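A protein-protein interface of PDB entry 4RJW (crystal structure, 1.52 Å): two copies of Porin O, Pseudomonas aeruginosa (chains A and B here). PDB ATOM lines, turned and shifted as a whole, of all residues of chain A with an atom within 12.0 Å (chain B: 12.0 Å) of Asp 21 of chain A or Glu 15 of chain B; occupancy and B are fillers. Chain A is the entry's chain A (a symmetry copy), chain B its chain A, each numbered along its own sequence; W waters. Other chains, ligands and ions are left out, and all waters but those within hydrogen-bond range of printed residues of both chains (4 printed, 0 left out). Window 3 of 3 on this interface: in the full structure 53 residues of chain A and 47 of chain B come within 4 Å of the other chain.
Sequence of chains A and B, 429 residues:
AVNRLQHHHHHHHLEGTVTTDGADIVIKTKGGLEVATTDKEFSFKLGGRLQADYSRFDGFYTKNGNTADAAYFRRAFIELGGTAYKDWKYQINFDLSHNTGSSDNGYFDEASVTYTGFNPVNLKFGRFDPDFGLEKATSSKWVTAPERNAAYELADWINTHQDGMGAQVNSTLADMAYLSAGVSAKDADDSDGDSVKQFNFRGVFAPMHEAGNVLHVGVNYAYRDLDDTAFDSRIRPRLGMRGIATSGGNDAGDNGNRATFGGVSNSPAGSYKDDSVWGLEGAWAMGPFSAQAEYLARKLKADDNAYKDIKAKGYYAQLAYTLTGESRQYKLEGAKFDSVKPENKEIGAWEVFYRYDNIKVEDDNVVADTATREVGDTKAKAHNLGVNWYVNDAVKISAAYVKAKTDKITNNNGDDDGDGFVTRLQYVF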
ATOM      1  N   THR A  17       4.844  -9.372  12.072  1.00  0.00           N
ATOM      2  CA  THR A  17       4.812  -8.784  13.416  1.00  0.00           C
ATOM      3  C   THR A  17       3.792  -7.669  13.572  1.00  0.00           C
ATOM      4  O   THR A  17       3.424  -7.006  12.605  1.00  0.00           O
ATOM      5  CB  THR A  17       6.176  -8.246  13.889  1.00  0.00           C
ATOM      6  OG1 THR A  17       6.514  -7.043  13.185  1.00  0.00           O
ATOM      7  CG2 THR A  17       7.285  -9.283  13.687  1.00  0.00           C
ATOM      8  N   VAL A  18       3.333  -7.489  14.806  1.00  0.00           N
ATOM      9  CA  VAL A  18       2.453  -6.382  15.159  1.00  0.00           C
ATOM     10  C   VAL A  18       3.072  -5.689  16.368  1.00  0.00           C
ATOM     11  O   VAL A  18       3.270  -6.301  17.416  1.00  0.00           O
ATOM     12  CB  VAL A  18       1.034  -6.859  15.498  1.00  0.00           C
ATOM     13  CG1 VAL A  18       0.156  -5.671  15.887  1.00  0.00           C
ATOM     14  CG2 VAL A  18       0.440  -7.596  14.313  1.00  0.00           C
ATOM     15  N   THR A  19       3.408  -4.417  16.207  1.00  0.00           N
ATOM     16  CA  THR A  19       4.091  -3.673  17.251  1.00  0.00           C
ATOM     17  C   THR A  19       3.453  -2.309  17.413  1.00  0.00           C
ATOM     18  O   THR A  19       2.498  -1.975  16.701  1.00  0.00           O
ATOM     19  CB  THR A  19       5.585  -3.476  16.922  1.00  0.00           C
ATOM     20  OG1 THR A  19       5.720  -2.817  15.655  1.00  0.00           O
ATOM     21  CG2 THR A  19       6.314  -4.820  16.875  1.00  0.00           C
ATOM     22  N   THR A  20       3.958  -1.528  18.362  1.00  0.00           N
ATOM     23  CA  THR A  20       3.502  -0.155  18.540  1.00  0.00           C
ATOM     24  C   THR A  20       4.706   0.735  18.823  1.00  0.00           C
ATOM     25  O   THR A  20       5.774   0.244  19.201  1.00  0.00           O
ATOM     26  CB  THR A  20       2.444  -0.032  19.666  1.00  0.00           C
ATOM     27  OG1 THR A  20       1.864   1.280  19.640  1.00  0.00           O
ATOM     28  CG2 THR A  20       3.051  -0.302  21.028  1.00  0.00           C
ATOM     29  N   ASP A  21       4.547   2.039  18.617  1.00  0.00           N
ATOM     30  CA  ASP A  21       5.648   2.960  18.859  1.00  0.00           C
ATOM     31  C   ASP A  21       5.566   3.583  20.245  1.00  0.00           C
ATOM     32  O   ASP A  21       6.512   4.224  20.694  1.00  0.00           O
ATOM     33  CB  ASP A  21       5.705   4.054  17.786  1.00  0.00           C
ATOM     34  CG  ASP A  21       4.491   4.972  17.815  1.00  0.00           C
ATOM     35  OD1 ASP A  21       3.403   4.527  18.229  1.00  0.00           O
ATOM     36  OD2 ASP A  21       4.629   6.150  17.419  1.00  0.00           O
ATOM     37  N   GLY A  22       4.439   3.397  20.920  1.00  0.00           N
ATOM     38  CA  GLY A  22       4.262   3.965  22.246  1.00  0.00           C
ATOM     39  C   GLY A  22       4.241   2.896  23.317  1.00  0.00           C
ATOM     40  O   GLY A  22       4.834   1.839  23.154  1.00  0.00           O
ATOM     41  N   ALA A  23       3.533   3.174  24.405  1.00  0.00           N
ATOM     42  CA  ALA A  23       3.346   2.215  25.486  1.00  0.00           C
ATOM     43  C   ALA A  23       2.724   0.921  24.977  1.00  0.00           C
ATOM     44  O   ALA A  23       1.912   0.940  24.041  1.00  0.00           O
ATOM     45  CB  ALA A  23       2.469   2.827  26.573  1.00  0.00           C
ATOM     46  N   ASP A  24       3.113  -0.196  25.590  1.00  0.00           N
ATOM     47  CA  ASP A  24       2.564  -1.513  25.258  1.00  0.00           C
ATOM     48  C   ASP A  24       1.043  -1.502  25.141  1.00  0.00           C
ATOM     49  O   ASP A  24       0.355  -0.901  25.961  1.00  0.00           O
ATOM     50  CB  ASP A  24       2.935  -2.542  26.331  1.00  0.00           C
ATOM     51  CG  ASP A  24       4.408  -2.914  26.326  1.00  0.00           C
ATOM     52  OD1 ASP A  24       5.171  -2.512  25.417  1.00  0.00           O
ATOM     53  OD2 ASP A  24       4.807  -3.643  27.260  1.00  0.00           O
ATOM     54  N   ILE A  25       0.527  -2.199  24.136  1.00  0.00           N
ATOM     55  CA  ILE A  25      -0.903  -2.240  23.883  1.00  0.00           C
ATOM     56  C   ILE A  25      -1.437  -3.658  24.065  1.00  0.00           C
ATOM     57  O   ILE A  25      -0.765  -4.633  23.727  1.00  0.00           O
ATOM     58  CB  ILE A  25      -1.206  -1.737  22.457  1.00  0.00           C
ATOM     59  CG1 ILE A  25      -1.181  -0.204  22.425  1.00  0.00           C
ATOM     60  CG2 ILE A  25      -2.563  -2.224  21.969  1.00  0.00           C
ATOM     61  CD1 ILE A  25      -1.277   0.371  21.028  1.00  0.00           C
ATOM     62  N   VAL A  26      -2.633  -3.760  24.627  1.00  0.00           N
ATOM     63  CA  VAL A  26      -3.369  -5.013  24.673  1.00  0.00           C
ATOM     64  C   VAL A  26      -4.602  -4.861  23.795  1.00  0.00           C
ATOM     65  O   VAL A  26      -5.328  -3.884  23.901  1.00  0.00           O
ATOM     66  CB  VAL A  26      -3.772  -5.374  26.112  1.00  0.00           C
ATOM     67  CG1 VAL A  26      -4.724  -6.563  26.125  1.00  0.00           C
ATOM     68  CG2 VAL A  26      -2.531  -5.680  26.939  1.00  0.00           C
ATOM     69  N   VAL A  35      -8.816  -1.753  22.272  1.00  0.00           N
ATOM     70  CA  VAL A  35      -7.375  -1.531  22.217  1.00  0.00           C
ATOM     71  C   VAL A  35      -7.028  -0.579  23.362  1.00  0.00           C
ATOM     72  O   VAL A  35      -7.723   0.417  23.580  1.00  0.00           O
ATOM     73  CB  VAL A  35      -6.967  -0.888  20.860  1.00  0.00           C
ATOM     74  CG1 VAL A  35      -5.463  -0.659  20.787  1.00  0.00           C
ATOM     75  CG2 VAL A  35      -7.427  -1.746  19.685  1.00  0.00           C
ATOM     76  N   ALA A  36      -5.986  -0.889  24.119  1.00  0.00           N
ATOM     77  CA  ALA A  36      -5.662  -0.047  25.256  1.00  0.00           C
ATOM     78  C   ALA A  36      -4.192  -0.143  25.582  1.00  0.00           C
ATOM     79  O   ALA A  36      -3.588  -1.214  25.447  1.00  0.00           O
ATOM     80  CB  ALA A  36      -6.484  -0.461  26.473  1.00  0.00           C
ATOM     81  N   THR A  37      -3.602   0.963  26.016  1.00  0.00           N
ATOM     82  CA  THR A  37      -2.250   0.885  26.542  1.00  0.00           C
ATOM     83  C   THR A  37      -2.257   0.315  27.954  1.00  0.00           C
ATOM     84  O   THR A  37      -3.180   0.536  28.735  1.00  0.00           O
ATOM     85  CB  THR A  37      -1.527   2.239  26.518  1.00  0.00           C
ATOM     86  OG1 THR A  37      -2.293   3.196  27.255  1.00  0.00           O
ATOM     87  CG2 THR A  37      -1.342   2.715  25.083  1.00  0.00           C
ATOM     88  N   THR A  38      -1.218  -0.441  28.276  1.00  0.00           N
ATOM     89  CA  THR A  38      -1.188  -1.127  29.554  1.00  0.00           C
ATOM     90  C   THR A  38      -1.041  -0.177  30.738  1.00  0.00           C
ATOM     91  O   THR A  38      -1.416  -0.519  31.860  1.00  0.00           O
ATOM     92  CB  THR A  38      -0.076  -2.182  29.572  1.00  0.00           C
ATOM     93  OG1 THR A  38       1.199  -1.553  29.390  1.00  0.00           O
ATOM     94  CG2 THR A  38      -0.312  -3.167  28.440  1.00  0.00           C
ATOM     95  N   ASP A  39      -0.489   1.007  30.487  1.00  0.00           N
ATOM     96  CA  ASP A  39      -0.347   2.024  31.527  1.00  0.00           C
ATOM     97  C   ASP A  39      -1.642   2.825  31.767  1.00  0.00           C
ATOM     98  O   ASP A  39      -1.628   3.818  32.503  1.00  0.00           O
ATOM     99  CB  ASP A  39       0.781   2.985  31.177  1.00  0.00           C
ATOM    100  CG  ASP A  39       0.551   3.714  29.864  1.00  0.00           C
ATOM    101  OD1 ASP A  39      -0.568   3.674  29.306  1.00  0.00           O
ATOM    102  OD2 ASP A  39       1.501   4.365  29.398  1.00  0.00           O
ATOM    103  N   LYS A  40      -2.729   2.411  31.118  1.00  0.00           N
ATOM    104  CA  LYS A  40      -4.055   3.018  31.298  1.00  0.00           C
ATOM    105  C   LYS A  40      -4.211   4.445  30.763  1.00  0.00           C
ATOM    106  O   LYS A  40      -5.237   5.086  31.001  1.00  0.00           O
ATOM    107  CB  LYS A  40      -4.500   2.967  32.768  1.00  0.00           C
ATOM    108  CG  LYS A  40      -4.417   1.588  33.402  1.00  0.00           C
ATOM    109  CD  LYS A  40      -5.279   0.588  32.653  1.00  0.00           C
ATOM    110  N   GLU A  41      -3.233   4.934  30.016  1.00  0.00           N
ATOM    111  CA  GLU A  41      -3.298   6.306  29.511  1.00  0.00           C
ATOM    112  C   GLU A  41      -4.288   6.451  28.362  1.00  0.00           C
ATOM    113  O   GLU A  41      -4.998   7.461  28.264  1.00  0.00           O
ATOM    114  CB  GLU A  41      -1.925   6.797  29.047  1.00  0.00           C
ATOM    115  CG  GLU A  41      -0.940   7.096  30.163  1.00  0.00           C
ATOM    116  CD  GLU A  41      -1.221   8.423  30.849  1.00  0.00           C
ATOM    117  OE1 GLU A  41      -1.584   9.393  30.147  1.00  0.00           O
ATOM    118  OE2 GLU A  41      -1.075   8.495  32.087  1.00  0.00           O
ATOM    119  N   PHE A  42      -4.347   5.448  27.492  1.00  0.00           N
ATOM    120  CA  PHE A  42      -5.139   5.545  26.274  1.00  0.00           C
ATOM    121  C   PHE A  42      -5.923   4.272  26.041  1.00  0.00           C
ATOM    122  O   PHE A  42      -5.423   3.173  26.266  1.00  0.00           O
ATOM    123  CB  PHE A  42      -4.242   5.812  25.058  1.00  0.00           C
ATOM    124  CG  PHE A  42      -3.483   7.106  25.135  1.00  0.00           C
ATOM    125  CD1 PHE A  42      -4.112   8.311  24.845  1.00  0.00           C
ATOM    126  CD2 PHE A  42      -2.144   7.119  25.501  1.00  0.00           C
ATOM    127  CE1 PHE A  42      -3.414   9.506  24.918  1.00  0.00           C
ATOM    128  CE2 PHE A  42      -1.443   8.310  25.569  1.00  0.00           C
ATOM    129  CZ  PHE A  42      -2.078   9.504  25.277  1.00  0.00           C
ATOM    130  N   TYR A  85      -5.072  10.454  27.853  1.00  0.00           N
ATOM    131  CA  TYR A  85      -4.362  11.088  28.957  1.00  0.00           C
ATOM    132  C   TYR A  85      -4.934  10.662  30.304  1.00  0.00           C
ATOM    133  O   TYR A  85      -5.038  11.463  31.240  1.00  0.00           O
ATOM    134  CB  TYR A  85      -4.318  12.607  28.766  1.00  0.00           C
ATOM    135  CG  TYR A  85      -3.675  12.929  27.445  1.00  0.00           C
ATOM    136  CD1 TYR A  85      -2.296  12.942  27.323  1.00  0.00           C
ATOM    137  CD2 TYR A  85      -4.440  13.148  26.309  1.00  0.00           C
ATOM    138  CE1 TYR A  85      -1.696  13.192  26.116  1.00  0.00           C
ATOM    139  CE2 TYR A  85      -3.845  13.406  25.089  1.00  0.00           C
ATOM    140  CZ  TYR A  85      -2.472  13.425  25.004  1.00  0.00           C
ATOM    141  OH  TYR A  85      -1.854  13.671  23.804  1.00  0.00           O
ATOM    142  N   HIS B  10       8.101  10.295  38.440  1.00  0.00           N
ATOM    143  CA  HIS B  10       8.213   9.904  37.049  1.00  0.00           C
ATOM    144  C   HIS B  10       7.968   8.409  36.907  1.00  0.00           C
ATOM    145  O   HIS B  10       8.496   7.610  37.679  1.00  0.00           O
ATOM    146  CB  HIS B  10       9.573  10.273  36.458  1.00  0.00           C
ATOM    147  CG  HIS B  10       9.660  10.024  34.985  1.00  0.00           C
ATOM    148  ND1 HIS B  10       8.917  10.738  34.072  1.00  0.00           N
ATOM    149  CD2 HIS B  10      10.381   9.129  34.268  1.00  0.00           C
ATOM    150  CE1 HIS B  10       9.177  10.297  32.853  1.00  0.00           C
ATOM    151  NE2 HIS B  10      10.059   9.319  32.944  1.00  0.00           N
ATOM    152  N   HIS B  11       7.151   8.045  35.925  1.00  0.00           N
ATOM    153  CA  HIS B  11       6.868   6.641  35.656  1.00  0.00           C
ATOM    154  C   HIS B  11       7.603   6.186  34.404  1.00  0.00           C
ATOM    155  O   HIS B  11       7.710   6.930  33.433  1.00  0.00           O
ATOM    156  CB  HIS B  11       5.366   6.413  35.464  1.00  0.00           C
ATOM    157  CG  HIS B  11       4.511   7.112  36.474  1.00  0.00           C
ATOM    158  ND1 HIS B  11       4.515   6.781  37.811  1.00  0.00           N
ATOM    159  CD2 HIS B  11       3.616   8.120  36.338  1.00  0.00           C
ATOM    160  CE1 HIS B  11       3.665   7.559  38.457  1.00  0.00           C
ATOM    161  NE2 HIS B  11       3.106   8.380  37.586  1.00  0.00           N
ATOM    162  N   HIS B  12       8.117   4.962  34.439  1.00  0.00           N
ATOM    163  CA  HIS B  12       8.675   4.339  33.251  1.00  0.00           C
ATOM    164  C   HIS B  12       7.621   3.398  32.685  1.00  0.00           C
ATOM    165  O   HIS B  12       7.003   2.632  33.422  1.00  0.00           O
ATOM    166  CB  HIS B  12       9.953   3.568  33.587  1.00  0.00           C
ATOM    167  N   HIS B  13       7.402   3.469  31.378  1.00  0.00           N
ATOM    168  CA  HIS B  13       6.433   2.598  30.733  1.00  0.00           C
ATOM    169  C   HIS B  13       7.129   1.642  29.775  1.00  0.00           C
ATOM    170  O   HIS B  13       7.999   2.046  29.006  1.00  0.00           O
ATOM    171  CB  HIS B  13       5.384   3.427  29.984  1.00  0.00           C
ATOM    172  CG  HIS B  13       4.608   4.358  30.866  1.00  0.00           C
ATOM    173  ND1 HIS B  13       3.937   5.456  30.376  1.00  0.00           N
ATOM    174  CD2 HIS B  13       4.396   4.347  32.202  1.00  0.00           C
ATOM    175  CE1 HIS B  13       3.343   6.088  31.379  1.00  0.00           C
ATOM    176  NE2 HIS B  13       3.607   5.433  32.495  1.00  0.00           N
ATOM    177  N   LEU B  14       6.756   0.371  29.841  1.00  0.00           N
ATOM    178  CA  LEU B  14       7.215  -0.597  28.855  1.00  0.00           C
ATOM    179  C   LEU B  14       6.589  -0.222  27.518  1.00  0.00           C
ATOM    180  O   LEU B  14       5.390   0.085  27.450  1.00  0.00           O
ATOM    181  CB  LEU B  14       6.814  -2.016  29.264  1.00  0.00           C
ATOM    182  CG  LEU B  14       7.566  -2.603  30.465  1.00  0.00           C
ATOM    183  CD1 LEU B  14       7.031  -3.978  30.832  1.00  0.00           C
ATOM    184  CD2 LEU B  14       9.057  -2.671  30.172  1.00  0.00           C
ATOM    185  N   GLU B  15       7.402  -0.234  26.466  1.00  0.00           N
ATOM    186  CA  GLU B  15       6.960   0.218  25.151  1.00  0.00           C
ATOM    187  C   GLU B  15       7.148  -0.829  24.060  1.00  0.00           C
ATOM    188  O   GLU B  15       8.005  -1.710  24.156  1.00  0.00           O
ATOM    189  CB  GLU B  15       7.705   1.497  24.764  1.00  0.00           C
ATOM    190  CG  GLU B  15       7.610   2.588  25.825  1.00  0.00           C
ATOM    191  CD  GLU B  15       7.865   3.976  25.281  1.00  0.00           C
ATOM    192  OE1 GLU B  15       7.854   4.933  26.084  1.00  0.00           O
ATOM    193  OE2 GLU B  15       8.068   4.117  24.057  1.00  0.00           O
ATOM    194  N   GLY B  16       6.315  -0.739  23.032  1.00  0.00           N
ATOM    195  CA  GLY B  16       6.572  -1.448  21.800  1.00  0.00           C
ATOM    196  C   GLY B  16       5.787  -2.713  21.534  1.00  0.00           C
ATOM    197  O   GLY B  16       5.628  -3.077  20.376  1.00  0.00           O
ATOM    198  N   THR B  17       5.311  -3.400  22.570  1.00  0.00           N
ATOM    199  CA  THR B  17       4.653  -4.686  22.318  1.00  0.00           C
ATOM    200  C   THR B  17       3.149  -4.580  22.139  1.00  0.00           C
ATOM    201  O   THR B  17       2.514  -3.657  22.645  1.00  0.00           O
ATOM    202  CB  THR B  17       4.926  -5.746  23.402  1.00  0.00           C
ATOM    203  OG1 THR B  17       4.219  -5.427  24.607  1.00  0.00           O
ATOM    204  CG2 THR B  17       6.424  -5.859  23.706  1.00  0.00           C
ATOM    205  N   VAL B  18       2.596  -5.533  21.397  1.00  0.00           N
ATOM    206  CA  VAL B  18       1.154  -5.659  21.235  1.00  0.00           C
ATOM    207  C   VAL B  18       0.792  -7.104  21.563  1.00  0.00           C
ATOM    208  O   VAL B  18       1.279  -8.039  20.930  1.00  0.00           O
ATOM    209  CB  VAL B  18       0.702  -5.320  19.807  1.00  0.00           C
ATOM    210  CG1 VAL B  18      -0.810  -5.491  19.675  1.00  0.00           C
ATOM    211  CG2 VAL B  18       1.111  -3.900  19.461  1.00  0.00           C
ATOM    212  N   THR B  19      -0.039  -7.284  22.580  1.00  0.00           N
ATOM    213  CA  THR B  19      -0.385  -8.614  23.052  1.00  0.00           C
ATOM    214  C   THR B  19      -1.879  -8.704  23.285  1.00  0.00           C
ATOM    215  O   THR B  19      -2.606  -7.725  23.079  1.00  0.00           O
ATOM    216  CB  THR B  19       0.336  -8.952  24.373  1.00  0.00           C
ATOM    217  OG1 THR B  19       0.024  -7.962  25.363  1.00  0.00           O
ATOM    218  CG2 THR B  19       1.850  -9.005  24.169  1.00  0.00           C
HETATM  219  O   HOH W   1       1.488  -5.600  25.152  1.00  0.00           O
HETATM  220  O   HOH W   2       3.364   0.383  29.267  1.00  0.00           O
HETATM  221  O   HOH W   3       2.794  -8.673  18.723  1.00  0.00           O
HETATM  222  O   HOH W   4       4.583  -7.361  20.177  1.00  0.00           O
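Val 18 of chain B touches its own counterpart, Val 18 of chain A. Thr 19 of chain A touches Val 18 of chain B, but with the chains exchanged Val 18 of chain A does not touch Thr 19 of chain B (6.2 Å). Positions printed for both chains: 17, 18 and 19.
Water W2 lies within hydrogen-bond range of O of Leu 14 of chain B (2.7 Å) and OG1 of Thr 38 of chain A (2.9 Å). Water W3 bridges the backbone carbonyl oxygen (O) of Val 18 of chain A (2.7 Å) and the backbone carbonyl oxygen (O) of Val 18 of chain B (2.8 Å). Water W1 lies within hydrogen-bond range of OG1 of Thr 19 of chain B (2.8 Å), OG1 of Thr 17 of chain B (2.8 Å) and O of Ile 25 of chain A (2.8 Å). Water W4 lies within hydrogen-bond range of N of Val 18 of chain B (3.0 Å) and O of Val 18 of chain A (3.2 Å).
N of Glu 15 of chain B sits close to OD1 of Asp 24 of chain A (3.4 Å). The backbone NH (N) of Thr 19 of chain B is in hydrogen-bond range of the backbone carbonyl oxygen (O) of Ile 25 of chain A (3.0 Å). The backbone NH of Asp 24 of chain A sits at hydrogen-bond distance from the backbone carbonyl oxygen of Leu 14 of chain B (3.0 Å). The backbone NH (N) of Ile 25 of chain A lies within hydrogen-bond range of the backbone carbonyl oxygen (O) of Thr 17 of chain B (2.9 Å). The backbone NH of Gly 16 of chain B lies within hydrogen-bond range of the backbone carbonyl oxygen of Gly 22 of chain A (3.0 Å). OD1 of Asp 24 of chain A sits at hydrogen-bond distance from N of Gly 16 of chain B (3.2 Å). The side-chain carboxylate of Asp 39 of chain A lies within hydrogen-bond range of a ring nitrogen (ND1) of His 13 of chain B. The backbone NH (N) of Thr 17 of chain B lies within hydrogen-bond range of the side-chain carboxylate (OD1) of Asp 24 of chain A. The backbone NH (N) of Thr 20 of chain A lies within hydrogen-bond range of the backbone carbonyl oxygen (O) of Gly 16 of chain B, 3.0 Å away.
Among the printed residues, pairs that only touch across the chains: Val 26 of chain A with Thr 19 of chain B (3.2 Å), Ile 25 of chain A with Val 18 of chain B (3.3 Å), Gly 22 of chain A with Glu 15 of chain B (3.3 Å), Thr 19 of chain A with Gly 16 of chain B (3.5 Å), Thr 19 of chain A with Val 18 of chain B (3.5 Å), Ala 23 of chain A with Leu 14 of chain B (3.5 Å), Val 18 of chain A with Val 18 of chain B (3.6 Å), Asp 21 of chain A with Glu 15 of chain B (3.7 Å), Thr 20 of chain A with Thr 17 of chain B (3.8 Å) and Thr 20 of chain A with Val 18 of chain B (3.9 Å).
Hydrophobic or aromatic side chains of chain B that line the printed part of chain A: His 13, Leu 14 and Val 18. Hydrophobic or aromatic side chains of chain A that line the printed part of chain B: Val 18 and Val 26. Among the printed residues, 19 pairs touch across the chains. Among the printed residues, no Asp or Glu carboxylate lies within 4 Å of a Lys or Arg side-chain nitrogen of the other chain.
Of the printed residues of chain B, Val 18 of chain A touches Val 18. Thr 19 of chain A touches just these residues of chain B: Gly 16 (3.5 Å) and Val 18 (3.5 Å). Gly 22 of chain A touches just these residues of chain B: Glu 15 (3.3 Å) and Gly 16 (3.0 Å). Of the printed residues of chain B, Val 26 of chain A touches Thr 19 (3.2 Å). Printed residues of chain B within 4 Å of Asp 39 of chain A: His 13 (2.8 Å). His 13 of chain B touches one residue of chain A. Glu 15 of chain B touches just these residues of chain A: Asp 21, Gly 22 and Asp 24. Of the printed residues of chain A, Gly 16 of chain B touches Thr 19, Thr 20, Gly 22 and Asp 24. Of the printed residues of chain A, Thr 17 of chain B touches Thr 20 (3.8 Å), Asp 24 (3.0 Å) and Ile 25 (2.9 Å). Printed residues of chain A within 4 Å of Val 18 of chain B: Val 18, Thr 19, Thr 20 and Ile 25. Printed residues of chain A within 4 Å of Thr 19 of chain B: Ile 25 and Val 26. The nearest residue of chain A that does not touch Glu 15 of chain B is Ala 23 of chain A (4.1 Å).
OG1 of Thr 37 of chain A sits at hydrogen-bond distance from OD1 of Asp 39 of chain A. N of Val 26 of chain A lies within hydrogen-bond range of O of Ala 36 of chain A (2.8 Å). The side-chain carboxylate (OD1) of Asp 39 of chain A sits at hydrogen-bond distance from the backbone NH (N) of Glu 41 of chain A (3.0 Å). The backbone carbonyl oxygen of Asp 24 of chain A is in hydrogen-bond range of the backbone NH of Thr 38 of chain A.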
